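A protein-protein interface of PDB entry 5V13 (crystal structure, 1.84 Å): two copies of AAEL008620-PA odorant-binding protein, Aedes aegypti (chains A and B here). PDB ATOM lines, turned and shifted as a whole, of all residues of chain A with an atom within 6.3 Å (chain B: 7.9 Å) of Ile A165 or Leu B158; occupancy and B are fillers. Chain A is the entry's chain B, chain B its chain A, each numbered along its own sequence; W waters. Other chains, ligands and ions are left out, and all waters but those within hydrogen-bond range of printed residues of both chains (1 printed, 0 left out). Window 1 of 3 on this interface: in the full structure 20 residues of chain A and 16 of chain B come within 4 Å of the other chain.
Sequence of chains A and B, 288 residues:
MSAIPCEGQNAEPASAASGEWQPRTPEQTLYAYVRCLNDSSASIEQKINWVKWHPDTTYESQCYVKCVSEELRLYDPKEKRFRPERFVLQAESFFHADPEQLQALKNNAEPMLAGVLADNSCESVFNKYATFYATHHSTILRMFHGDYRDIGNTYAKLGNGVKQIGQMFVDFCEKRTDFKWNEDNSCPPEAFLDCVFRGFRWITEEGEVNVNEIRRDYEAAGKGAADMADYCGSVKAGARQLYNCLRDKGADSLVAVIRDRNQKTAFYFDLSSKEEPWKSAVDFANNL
Among the printed residues, merely in contact across the chains: Ile A151 with Asn B153 (3.5 Å), Ile A151 with Ala B156 (3.8 Å), Gln A164 with Asn B160 (3.8 Å), Ile A165 with Ala B156 (3.6 Å), Ile A165 with Lys B157 (3.8 Å), Ile A165 with Leu B158 (3.99 Å), Ile A165 with Gly B159 (3.3 Å), Gly A166 with Asn B160 (3.5 Å), Gln A167 with Asn B160 (3.3 Å) and Leu A271 with Lys B157 (3.8 Å).
NE2 of Gln B164 is in hydrogen-bond range of O of Gly B159.
N of Gln A164 is in hydrogen-bond range of OE1 of Gln A167, at 3.1 Å.
The side-chain amino group of Lys B157 sits at hydrogen-bond distance from the backbone carbonyl oxygen of Ser B93 (3.1 Å).
The side-chain amino group of Lys A163 is in hydrogen-bond range of the backbone carbonyl oxygen of Gln A167 (2.9 Å).
N of Gly A166 is in hydrogen-bond range of O of Ala A266.
Of the 24 printed residues of chain B, 6 touch a printed residue of chain A.
Printed residues of chain B that touch a printed residue of chain A: Asn B153, Ala B156, Lys B157, Leu B158, Gly B159 and Asn B160.
Of the 11 printed residues of chain A, 6 touch a printed residue of chain B.
Along chain A the printed residues that touch a printed residue of chain B span positions 151 to 271.
The backbone NH of Asn B160 lies within hydrogen-bond range of the backbone carbonyl oxygen of Ile A165, 2.7 Å away.
Water W1 lies within hydrogen-bond range of O of Ala B156 (2.8 Å), OE1 of Gln A164 (3.0 Å) and N of Ile A165 (3.0 Å).
Printed residues of chain B within 4 Å of Ile A165: Ala B156, Lys B157, Leu B158, Gly B159 and Asn B160.
Of the printed residues of chain A, Leu B158 touches Ile A165 (3.99 Å).
Printed residues of chain A within 4 Å of Gly B159: Ile A165.
Printed residues of chain A within 4 Å of Lys B157: Ile A165 and Leu A271.
Of the printed residues of chain A, Asn B153 touches Ile A151.
Of the printed residues of chain A, Asn B160 touches Gln A164 (3.8 Å), Ile A165 (2.7 Å), Gly A166 (3.5 Å) and Gln A167 (3.3 Å).
Leu A30 touches none of the printed residues of chain B.
The nearest printed residue of chain A that does not touch Leu B158 is Phe A267 (4.8 Å).
3 positions are printed for both chains.
Of the 11 pairs that touch across the chains among the printed residues, none has its exchanged pair printed and touching as well.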
ATOM      1  N   LEU A  30      20.233  32.412 -32.285  1.00  0.00           N
ATOM      2  CA  LEU A  30      20.481  33.351 -31.191  1.00  0.00           C
ATOM      3  C   LEU A  30      21.005  34.691 -31.717  1.00  0.00           C
ATOM      4  O   LEU A  30      20.599  35.757 -31.235  1.00  0.00           O
ATOM      5  CB  LEU A  30      21.444  32.740 -30.173  1.00  0.00           C
ATOM      6  CG  LEU A  30      21.523  33.456 -28.819  1.00  0.00           C
ATOM      7  CD1 LEU A  30      20.158  33.511 -28.119  1.00  0.00           C
ATOM      8  CD2 LEU A  30      22.556  32.798 -27.936  1.00  0.00           C
ATOM      9  N   ILE A 151      18.606  21.439 -25.921  1.00  0.00           N
ATOM     10  CA  ILE A 151      19.821  22.199 -26.212  1.00  0.00           C
ATOM     11  C   ILE A 151      21.052  21.291 -26.182  1.00  0.00           C
ATOM     12  O   ILE A 151      21.982  21.457 -26.988  1.00  0.00           O
ATOM     13  CB  ILE A 151      19.950  23.399 -25.252  1.00  0.00           C
ATOM     14  CG1 ILE A 151      21.083  24.320 -25.712  1.00  0.00           C
ATOM     15  CG2 ILE A 151      20.159  22.950 -23.803  1.00  0.00           C
ATOM     16  CD1 ILE A 151      21.021  25.736 -25.101  1.00  0.00           C
ATOM     17  N   TYR A 155      23.539  20.896 -29.530  1.00  0.00           N
ATOM     18  CA  TYR A 155      24.935  21.321 -29.586  1.00  0.00           C
ATOM     19  C   TYR A 155      25.885  20.128 -29.677  1.00  0.00           C
ATOM     20  O   TYR A 155      26.984  20.268 -30.218  1.00  0.00           O
ATOM     21  CB  TYR A 155      25.293  22.196 -28.380  1.00  0.00           C
ATOM     22  CG  TYR A 155      24.969  23.667 -28.561  1.00  0.00           C
ATOM     23  CD1 TYR A 155      25.819  24.510 -29.291  1.00  0.00           C
ATOM     24  CD2 TYR A 155      23.820  24.218 -28.000  1.00  0.00           C
ATOM     25  CE1 TYR A 155      25.520  25.874 -29.449  1.00  0.00           C
ATOM     26  CE2 TYR A 155      23.524  25.568 -28.146  1.00  0.00           C
ATOM     27  CZ  TYR A 155      24.372  26.388 -28.875  1.00  0.00           C
ATOM     28  OH  TYR A 155      24.070  27.726 -29.026  1.00  0.00           O
ATOM     29  N   LYS A 163      29.950  27.278 -33.336  1.00  0.00           N
ATOM     30  CA  LYS A 163      30.428  28.046 -32.189  1.00  0.00           C
ATOM     31  C   LYS A 163      29.515  27.813 -30.990  1.00  0.00           C
ATOM     32  O   LYS A 163      28.298  27.998 -31.077  1.00  0.00           O
ATOM     33  CB  LYS A 163      30.487  29.544 -32.513  1.00  0.00           C
ATOM     34  CG  LYS A 163      31.126  30.363 -31.387  1.00  0.00           C
ATOM     35  CD  LYS A 163      30.902  31.860 -31.567  1.00  0.00           C
ATOM     36  CE  LYS A 163      29.538  32.248 -31.023  1.00  0.00           C
ATOM     37  NZ  LYS A 163      29.515  32.195 -29.525  1.00  0.00           N
ATOM     38  N   GLN A 164      30.105  27.425 -29.862  1.00  0.00           N
ATOM     39  CA  GLN A 164      29.334  27.123 -28.667  1.00  0.00           C
ATOM     40  C   GLN A 164      29.038  28.396 -27.877  1.00  0.00           C
ATOM     41  O   GLN A 164      29.678  29.436 -28.058  1.00  0.00           O
ATOM     42  CB  GLN A 164      30.070  26.114 -27.783  1.00  0.00           C
ATOM     43  CG  GLN A 164      30.434  24.779 -28.478  1.00  0.00           C
ATOM     44  CD  GLN A 164      29.298  23.761 -28.474  1.00  0.00           C
ATOM     45  OE1 GLN A 164      28.585  23.619 -27.476  1.00  0.00           O
ATOM     46  NE2 GLN A 164      29.117  23.053 -29.599  1.00  0.00           N
ATOM     47  N   ILE A 165      28.030  28.307 -27.007  1.00  0.00           N
ATOM     48  CA  ILE A 165      27.758  29.392 -26.067  1.00  0.00           C
ATOM     49  C   ILE A 165      29.018  29.643 -25.254  1.00  0.00           C
ATOM     50  O   ILE A 165      29.621  28.706 -24.717  1.00  0.00           O
ATOM     51  CB  ILE A 165      26.567  29.034 -25.163  1.00  0.00           C
ATOM     52  CG1 ILE A 165      25.271  29.010 -25.972  1.00  0.00           C
ATOM     53  CG2 ILE A 165      26.441  30.032 -23.982  1.00  0.00           C
ATOM     54  CD1 ILE A 165      24.112  28.328 -25.230  1.00  0.00           C
ATOM     55  N   GLY A 166      29.441  30.910 -25.186  1.00  0.00           N
ATOM     56  CA  GLY A 166      30.640  31.273 -24.453  1.00  0.00           C
ATOM     57  C   GLY A 166      31.949  31.120 -25.212  1.00  0.00           C
ATOM     58  O   GLY A 166      32.998  31.506 -24.684  1.00  0.00           O
ATOM     59  N   GLN A 167      31.939  30.554 -26.412  1.00  0.00           N
ATOM     60  CA  GLN A 167      33.149  30.454 -27.222  1.00  0.00           C
ATOM     61  C   GLN A 167      33.277  31.681 -28.125  1.00  0.00           C
ATOM     62  O   GLN A 167      32.293  32.137 -28.702  1.00  0.00           O
ATOM     63  CB  GLN A 167      33.122  29.174 -28.067  1.00  0.00           C
ATOM     64  CG  GLN A 167      34.332  28.983 -28.994  1.00  0.00           C
ATOM     65  CD  GLN A 167      34.284  27.672 -29.769  1.00  0.00           C
ATOM     66  OE1 GLN A 167      33.203  27.174 -30.097  1.00  0.00           O
ATOM     67  NE2 GLN A 167      35.464  27.123 -30.099  1.00  0.00           N
ATOM     68  N   ALA A 266      31.454  35.881 -27.555  1.00  0.00           N
ATOM     69  CA  ALA A 266      31.309  34.754 -26.635  1.00  0.00           C
ATOM     70  C   ALA A 266      29.860  34.574 -26.199  1.00  0.00           C
ATOM     71  O   ALA A 266      29.273  33.499 -26.378  1.00  0.00           O
ATOM     72  CB  ALA A 266      32.213  34.951 -25.417  1.00  0.00           C
ATOM     73  N   PHE A 267      29.269  35.612 -25.594  1.00  0.00           N
ATOM     74  CA  PHE A 267      27.905  35.560 -25.075  1.00  0.00           C
ATOM     75  C   PHE A 267      27.069  36.631 -25.766  1.00  0.00           C
ATOM     76  O   PHE A 267      27.223  37.823 -25.482  1.00  0.00           O
ATOM     77  CB  PHE A 267      27.878  35.766 -23.565  1.00  0.00           C
ATOM     78  CG  PHE A 267      28.746  34.807 -22.800  1.00  0.00           C
ATOM     79  CD1 PHE A 267      28.266  33.555 -22.451  1.00  0.00           C
ATOM     80  CD2 PHE A 267      30.040  35.161 -22.425  1.00  0.00           C
ATOM     81  CE1 PHE A 267      29.056  32.675 -21.735  1.00  0.00           C
ATOM     82  CE2 PHE A 267      30.838  34.282 -21.713  1.00  0.00           C
ATOM     83  CZ  PHE A 267      30.344  33.040 -21.368  1.00  0.00           C
ATOM     84  N   LEU A 271      22.897  34.833 -20.170  1.00  0.00           N
ATOM     85  CA  LEU A 271      21.798  33.942 -19.801  1.00  0.00           C
ATOM     86  C   LEU A 271      21.487  33.971 -18.307  1.00  0.00           C
ATOM     87  O   LEU A 271      20.461  33.417 -17.890  1.00  0.00           O
ATOM     88  CB  LEU A 271      22.094  32.500 -20.238  1.00  0.00           C
ATOM     89  CG  LEU A 271      21.512  32.055 -21.588  1.00  0.00           C
ATOM     90  CD1 LEU A 271      22.178  32.806 -22.728  1.00  0.00           C
ATOM     91  CD2 LEU A 271      21.623  30.543 -21.792  1.00  0.00           C
ATOM     92  N   PRO B  23      24.165  30.702  -9.333  1.00  0.00           N
ATOM     93  CA  PRO B  23      23.833  29.271  -9.255  1.00  0.00           C
ATOM     94  C   PRO B  23      25.064  28.408  -9.490  1.00  0.00           C
ATOM     95  O   PRO B  23      25.890  28.694 -10.364  1.00  0.00           O
ATOM     96  CB  PRO B  23      22.793  29.086 -10.374  1.00  0.00           C
ATOM     97  CG  PRO B  23      22.168  30.433 -10.511  1.00  0.00           C
ATOM     98  CD  PRO B  23      23.274  31.424 -10.258  1.00  0.00           C
ATOM     99  N   ARG B  24      25.204  27.366  -8.665  1.00  0.00           N
ATOM    100  CA  ARG B  24      26.354  26.480  -8.754  1.00  0.00           C
ATOM    101  C   ARG B  24      26.329  25.726 -10.077  1.00  0.00           C
ATOM    102  O   ARG B  24      25.317  25.113 -10.432  1.00  0.00           O
ATOM    103  CB  ARG B  24      26.339  25.483  -7.591  1.00  0.00           C
ATOM    104  CG  ARG B  24      26.322  26.134  -6.171  1.00  0.00           C
ATOM    105  CD  ARG B  24      27.578  26.971  -5.889  1.00  0.00           C
ATOM    106  NE  ARG B  24      27.497  28.364  -6.339  1.00  0.00           N
ATOM    107  CZ  ARG B  24      28.400  29.293  -6.027  1.00  0.00           C
ATOM    108  NH1 ARG B  24      29.442  28.976  -5.266  1.00  0.00           N
ATOM    109  NH2 ARG B  24      28.262  30.542  -6.454  1.00  0.00           N
ATOM    110  N   THR B  25      27.451  25.752 -10.788  1.00  0.00           N
ATOM    111  CA  THR B  25      27.636  24.941 -11.991  1.00  0.00           C
ATOM    112  C   THR B  25      27.920  23.493 -11.619  1.00  0.00           C
ATOM    113  O   THR B  25      28.215  23.187 -10.463  1.00  0.00           O
ATOM    114  CB  THR B  25      28.804  25.481 -12.801  1.00  0.00           C
ATOM    115  OG1 THR B  25      30.013  25.256 -12.065  1.00  0.00           O
ATOM    116  CG2 THR B  25      28.625  26.960 -13.090  1.00  0.00           C
ATOM    117  N   PRO B  26      27.867  22.573 -12.592  1.00  0.00           N
ATOM    118  CA  PRO B  26      28.311  21.195 -12.309  1.00  0.00           C
ATOM    119  C   PRO B  26      29.792  21.100 -11.994  1.00  0.00           C
ATOM    120  O   PRO B  26      30.199  20.148 -11.326  1.00  0.00           O
ATOM    121  CB  PRO B  26      27.950  20.429 -13.596  1.00  0.00           C
ATOM    122  CG  PRO B  26      27.754  21.488 -14.648  1.00  0.00           C
ATOM    123  CD  PRO B  26      27.226  22.685 -13.918  1.00  0.00           C
ATOM    124  N   GLU B  27      30.615  22.056 -12.441  1.00  0.00           N
ATOM    125  CA  GLU B  27      32.004  22.063 -11.988  1.00  0.00           C
ATOM    126  C   GLU B  27      32.069  22.337 -10.491  1.00  0.00           C
ATOM    127  O   GLU B  27      32.813  21.679  -9.761  1.00  0.00           O
ATOM    128  CB  GLU B  27      32.822  23.106 -12.759  1.00  0.00           C
ATOM    129  CG  GLU B  27      34.328  23.149 -12.410  1.00  0.00           C
ATOM    130  CD  GLU B  27      34.661  23.897 -11.114  1.00  0.00           C
ATOM    131  OE1 GLU B  27      35.670  23.525 -10.443  1.00  0.00           O
ATOM    132  OE2 GLU B  27      33.940  24.877 -10.785  1.00  0.00           O
ATOM    133  N   GLN B  28      31.279  23.299 -10.019  1.00  0.00           N
ATOM    134  CA  GLN B  28      31.306  23.671  -8.607  1.00  0.00           C
ATOM    135  C   GLN B  28      30.715  22.575  -7.708  1.00  0.00           C
ATOM    136  O   GLN B  28      31.272  22.271  -6.645  1.00  0.00           O
ATOM    137  CB  GLN B  28      30.572  25.002  -8.440  1.00  0.00           C
ATOM    138  CG  GLN B  28      31.416  26.188  -8.958  1.00  0.00           C
ATOM    139  CD  GLN B  28      30.650  27.494  -8.950  1.00  0.00           C
ATOM    140  OE1 GLN B  28      29.489  27.551  -9.372  1.00  0.00           O
ATOM    141  NE2 GLN B  28      31.299  28.553  -8.487  1.00  0.00           N
ATOM    142  N   SER B  93      17.172  28.256 -11.738  1.00  0.00           N
ATOM    143  CA  SER B  93      18.070  28.044 -12.864  1.00  0.00           C
ATOM    144  C   SER B  93      18.038  26.611 -13.378  1.00  0.00           C
ATOM    145  O   SER B  93      18.183  26.392 -14.587  1.00  0.00           O
ATOM    146  CB  SER B  93      19.502  28.426 -12.477  1.00  0.00           C
ATOM    147  OG  SER B  93      20.406  28.107 -13.526  1.00  0.00           O
ATOM    148  N   PHE B  94      17.868  25.621 -12.494  1.00  0.00           N
ATOM    149  CA  PHE B  94      18.161  24.236 -12.858  1.00  0.00           C
ATOM    150  C   PHE B  94      17.071  23.212 -12.561  1.00  0.00           C
ATOM    151  O   PHE B  94      17.306  22.019 -12.784  1.00  0.00           O
ATOM    152  CB  PHE B  94      19.451  23.756 -12.174  1.00  0.00           C
ATOM    153  CG  PHE B  94      20.717  24.398 -12.716  1.00  0.00           C
ATOM    154  CD1 PHE B  94      21.099  24.211 -14.039  1.00  0.00           C
ATOM    155  CD2 PHE B  94      21.523  25.171 -11.897  1.00  0.00           C
ATOM    156  CE1 PHE B  94      22.252  24.812 -14.541  1.00  0.00           C
ATOM    157  CE2 PHE B  94      22.687  25.756 -12.379  1.00  0.00           C
ATOM    158  CZ  PHE B  94      23.054  25.574 -13.711  1.00  0.00           C
ATOM    159  N   HIS B 145      22.590  19.103  -9.779  1.00  0.00           N
ATOM    160  CA  HIS B 145      23.276  18.318 -10.805  1.00  0.00           C
ATOM    161  C   HIS B 145      23.471  16.860 -10.411  1.00  0.00           C
ATOM    162  O   HIS B 145      24.384  16.190 -10.911  1.00  0.00           O
ATOM    163  CB  HIS B 145      24.604  18.977 -11.174  1.00  0.00           C
ATOM    164  CG  HIS B 145      24.464  20.448 -11.400  1.00  0.00           C
ATOM    165  ND1 HIS B 145      23.545  20.971 -12.284  1.00  0.00           N
ATOM    166  CD2 HIS B 145      25.062  21.508 -10.802  1.00  0.00           C
ATOM    167  CE1 HIS B 145      23.604  22.291 -12.246  1.00  0.00           C
ATOM    168  NE2 HIS B 145      24.522  22.642 -11.361  1.00  0.00           N
ATOM    169  N   GLY B 152      23.587  16.664 -20.275  1.00  0.00           N
ATOM    170  CA  GLY B 152      23.792  17.244 -21.594  1.00  0.00           C
ATOM    171  C   GLY B 152      23.244  18.655 -21.702  1.00  0.00           C
ATOM    172  O   GLY B 152      23.932  19.569 -22.169  1.00  0.00           O
ATOM    173  N   ASN B 153      21.987  18.848 -21.283  1.00  0.00           N
ATOM    174  CA  ASN B 153      21.369  20.179 -21.340  1.00  0.00           C
ATOM    175  C   ASN B 153      22.131  21.188 -20.491  1.00  0.00           C
ATOM    176  O   ASN B 153      22.369  22.325 -20.918  1.00  0.00           O
ATOM    177  CB  ASN B 153      19.913  20.097 -20.873  1.00  0.00           C
ATOM    178  CG  ASN B 153      19.011  19.472 -21.893  1.00  0.00           C
ATOM    179  OD1 ASN B 153      19.325  19.459 -23.082  1.00  0.00           O
ATOM    180  ND2 ASN B 153      17.871  18.956 -21.444  1.00  0.00           N
ATOM    181  N   THR B 154      22.522  20.784 -19.283  1.00  0.00           N
ATOM    182  CA  THR B 154      23.209  21.684 -18.362  1.00  0.00           C
ATOM    183  C   THR B 154      24.545  22.161 -18.928  1.00  0.00           C
ATOM    184  O   THR B 154      24.857  23.359 -18.888  1.00  0.00           O
ATOM    185  CB  THR B 154      23.408  20.974 -17.021  1.00  0.00           C
ATOM    186  OG1 THR B 154      22.129  20.666 -16.444  1.00  0.00           O
ATOM    187  CG2 THR B 154      24.236  21.828 -16.063  1.00  0.00           C
ATOM    188  N   TYR B 155      25.364  21.240 -19.445  1.00  0.00           N
ATOM    189  CA  TYR B 155      26.671  21.675 -19.939  1.00  0.00           C
ATOM    190  C   TYR B 155      26.558  22.425 -21.270  1.00  0.00           C
ATOM    191  O   TYR B 155      27.418  23.261 -21.580  1.00  0.00           O
ATOM    192  CB  TYR B 155      27.634  20.484 -20.071  1.00  0.00           C
ATOM    193  CG  TYR B 155      28.409  20.162 -18.800  1.00  0.00           C
ATOM    194  CD1 TYR B 155      29.547  20.895 -18.447  1.00  0.00           C
ATOM    195  CD2 TYR B 155      28.022  19.118 -17.967  1.00  0.00           C
ATOM    196  CE1 TYR B 155      30.278  20.587 -17.292  1.00  0.00           C
ATOM    197  CE2 TYR B 155      28.738  18.816 -16.800  1.00  0.00           C
ATOM    198  CZ  TYR B 155      29.861  19.553 -16.468  1.00  0.00           C
ATOM    199  OH  TYR B 155      30.578  19.250 -15.316  1.00  0.00           O
ATOM    200  N   ALA B 156      25.519  22.162 -22.064  1.00  0.00           N
ATOM    201  CA  ALA B 156      25.391  22.912 -23.314  1.00  0.00           C
ATOM    202  C   ALA B 156      24.838  24.323 -23.089  1.00  0.00           C
ATOM    203  O   ALA B 156      25.247  25.259 -23.785  1.00  0.00           O
ATOM    204  CB  ALA B 156      24.515  22.151 -24.308  1.00  0.00           C
ATOM    205  N   LYS B 157      23.943  24.495 -22.107  1.00  0.00           N
ATOM    206  CA  LYS B 157      23.446  25.832 -21.772  1.00  0.00           C
ATOM    207  C   LYS B 157      24.564  26.705 -21.229  1.00  0.00           C
ATOM    208  O   LYS B 157      24.604  27.909 -21.488  1.00  0.00           O
ATOM    209  CB  LYS B 157      22.303  25.721 -20.760  1.00  0.00           C
ATOM    210  CG  LYS B 157      21.659  27.047 -20.379  1.00  0.00           C
ATOM    211  CD  LYS B 157      20.644  26.886 -19.235  1.00  0.00           C
ATOM    212  CE  LYS B 157      21.331  26.668 -17.878  1.00  0.00           C
ATOM    213  NZ  LYS B 157      20.375  26.695 -16.717  1.00  0.00           N
ATOM    214  N   LEU B 158      25.468  26.122 -20.449  1.00  0.00           N
ATOM    215  CA  LEU B 158      26.618  26.866 -19.953  1.00  0.00           C
ATOM    216  C   LEU B 158      27.736  26.968 -20.988  1.00  0.00           C
ATOM    217  O   LEU B 158      28.493  27.944 -20.967  1.00  0.00           O
ATOM    218  CB  LEU B 158      27.142  26.217 -18.668  1.00  0.00           C
ATOM    219  CG  LEU B 158      26.166  26.161 -17.493  1.00  0.00           C
ATOM    220  CD1 LEU B 158      26.739  25.326 -16.332  1.00  0.00           C
ATOM    221  CD2 LEU B 158      25.826  27.582 -17.021  1.00  0.00           C
ATOM    222  N   GLY B 159      27.877  25.969 -21.865  1.00  0.00           N
ATOM    223  CA  GLY B 159      28.884  25.991 -22.922  1.00  0.00           C
ATOM    224  C   GLY B 159      30.296  26.195 -22.403  1.00  0.00           C
ATOM    225  O   GLY B 159      30.710  25.632 -21.378  1.00  0.00           O
ATOM    226  N   ASN B 160      31.052  27.032 -23.115  1.00  0.00           N
ATOM    227  CA  ASN B 160      32.394  27.417 -22.693  1.00  0.00           C
ATOM    228  C   ASN B 160      32.391  28.367 -21.514  1.00  0.00           C
ATOM    229  O   ASN B 160      33.471  28.811 -21.107  1.00  0.00           O
ATOM    230  CB  ASN B 160      33.158  28.081 -23.838  1.00  0.00           C
ATOM    231  CG  ASN B 160      33.507  27.122 -24.947  1.00  0.00           C
ATOM    232  OD1 ASN B 160      32.849  26.103 -25.148  1.00  0.00           O
ATOM    233  ND2 ASN B 160      34.555  27.452 -25.687  1.00  0.00           N
ATOM    234  N   GLY B 161      31.229  28.712 -20.964  1.00  0.00           N
ATOM    235  CA  GLY B 161      31.227  29.434 -19.704  1.00  0.00           C
ATOM    236  C   GLY B 161      31.537  28.597 -18.477  1.00  0.00           C
ATOM    237  O   GLY B 161      31.666  29.154 -17.384  1.00  0.00           O
ATOM    238  N   VAL B 162      31.623  27.274 -18.612  1.00  0.00           N
ATOM    239  CA  VAL B 162      31.960  26.392 -17.497  1.00  0.00           C
ATOM    240  C   VAL B 162      33.058  25.449 -17.957  1.00  0.00           C
ATOM    241  O   VAL B 162      33.107  25.062 -19.128  1.00  0.00           O
ATOM    242  CB  VAL B 162      30.728  25.589 -16.991  1.00  0.00           C
ATOM    243  CG1 VAL B 162      30.300  24.548 -18.019  1.00  0.00           C
ATOM    244  CG2 VAL B 162      31.019  24.922 -15.663  1.00  0.00           C
ATOM    245  N   LYS B 163      33.965  25.103 -17.042  1.00  0.00           N
ATOM    246  CA  LYS B 163      34.971  24.094 -17.372  1.00  0.00           C
ATOM    247  C   LYS B 163      34.289  22.745 -17.562  1.00  0.00           C
ATOM    248  O   LYS B 163      33.540  22.288 -16.695  1.00  0.00           O
ATOM    249  CB  LYS B 163      36.037  24.003 -16.278  1.00  0.00           C
ATOM    250  CG  LYS B 163      37.201  23.056 -16.608  1.00  0.00           C
ATOM    251  CD  LYS B 163      38.014  22.733 -15.348  1.00  0.00           C
ATOM    252  CE  LYS B 163      37.305  21.684 -14.480  1.00  0.00           C
ATOM    253  NZ  LYS B 163      37.319  20.347 -15.128  1.00  0.00           N
ATOM    254  N   GLN B 164      34.543  22.105 -18.701  1.00  0.00           N
ATOM    255  CA  GLN B 164      33.886  20.844 -18.988  1.00  0.00           C
ATOM    256  C   GLN B 164      34.615  19.696 -18.293  1.00  0.00           C
ATOM    257  O   GLN B 164      35.766  19.819 -17.869  1.00  0.00           O
ATOM    258  CB  GLN B 164      33.832  20.592 -20.498  1.00  0.00           C
ATOM    259  CG  GLN B 164      33.098  21.698 -21.290  1.00  0.00           C
ATOM    260  CD  GLN B 164      31.583  21.582 -21.232  1.00  0.00           C
ATOM    261  OE1 GLN B 164      31.028  20.478 -21.302  1.00  0.00           O
ATOM    262  NE2 GLN B 164      30.897  22.732 -21.104  1.00  0.00           N
ATOM    263  N   PHE B 172      40.742  26.327 -20.107  1.00  0.00           N
ATOM    264  CA  PHE B 172      39.486  27.056 -19.945  1.00  0.00           C
ATOM    265  C   PHE B 172      39.741  28.549 -19.769  1.00  0.00           C
ATOM    266  O   PHE B 172      39.070  29.388 -20.385  1.00  0.00           O
ATOM    267  CB  PHE B 172      38.724  26.481 -18.747  1.00  0.00           C
ATOM    268  CG  PHE B 172      37.528  27.275 -18.353  1.00  0.00           C
ATOM    269  CD1 PHE B 172      36.301  27.061 -18.975  1.00  0.00           C
ATOM    270  CD2 PHE B 172      37.613  28.237 -17.356  1.00  0.00           C
ATOM    271  CE1 PHE B 172      35.194  27.812 -18.618  1.00  0.00           C
ATOM    272  CE2 PHE B 172      36.508  28.981 -16.994  1.00  0.00           C
ATOM    273  CZ  PHE B 172      35.294  28.765 -17.633  1.00  0.00           C
ATOM    274  N   ARG B 176      38.731  31.822 -22.185  1.00  0.00           N
ATOM    275  CA  ARG B 176      37.812  32.821 -21.639  1.00  0.00           C
ATOM    276  C   ARG B 176      38.389  34.224 -21.715  1.00  0.00           C
ATOM    277  O   ARG B 176      37.641  35.197 -21.888  1.00  0.00           O
ATOM    278  CB  ARG B 176      37.472  32.463 -20.183  1.00  0.00           C
ATOM    279  CG  ARG B 176      36.596  33.473 -19.446  1.00  0.00           C
ATOM    280  CD  ARG B 176      36.253  32.951 -18.052  1.00  0.00           C
ATOM    281  NE  ARG B 176      35.367  33.851 -17.319  1.00  0.00           N
ATOM    282  CZ  ARG B 176      34.038  33.779 -17.341  1.00  0.00           C
ATOM    283  NH1 ARG B 176      33.428  32.850 -18.067  1.00  0.00           N
ATOM    284  NH2 ARG B 176      33.318  34.638 -16.631  1.00  0.00           N
HETATM  285  O   HOH W   1      27.012  25.632 -25.959  1.00  0.00           O
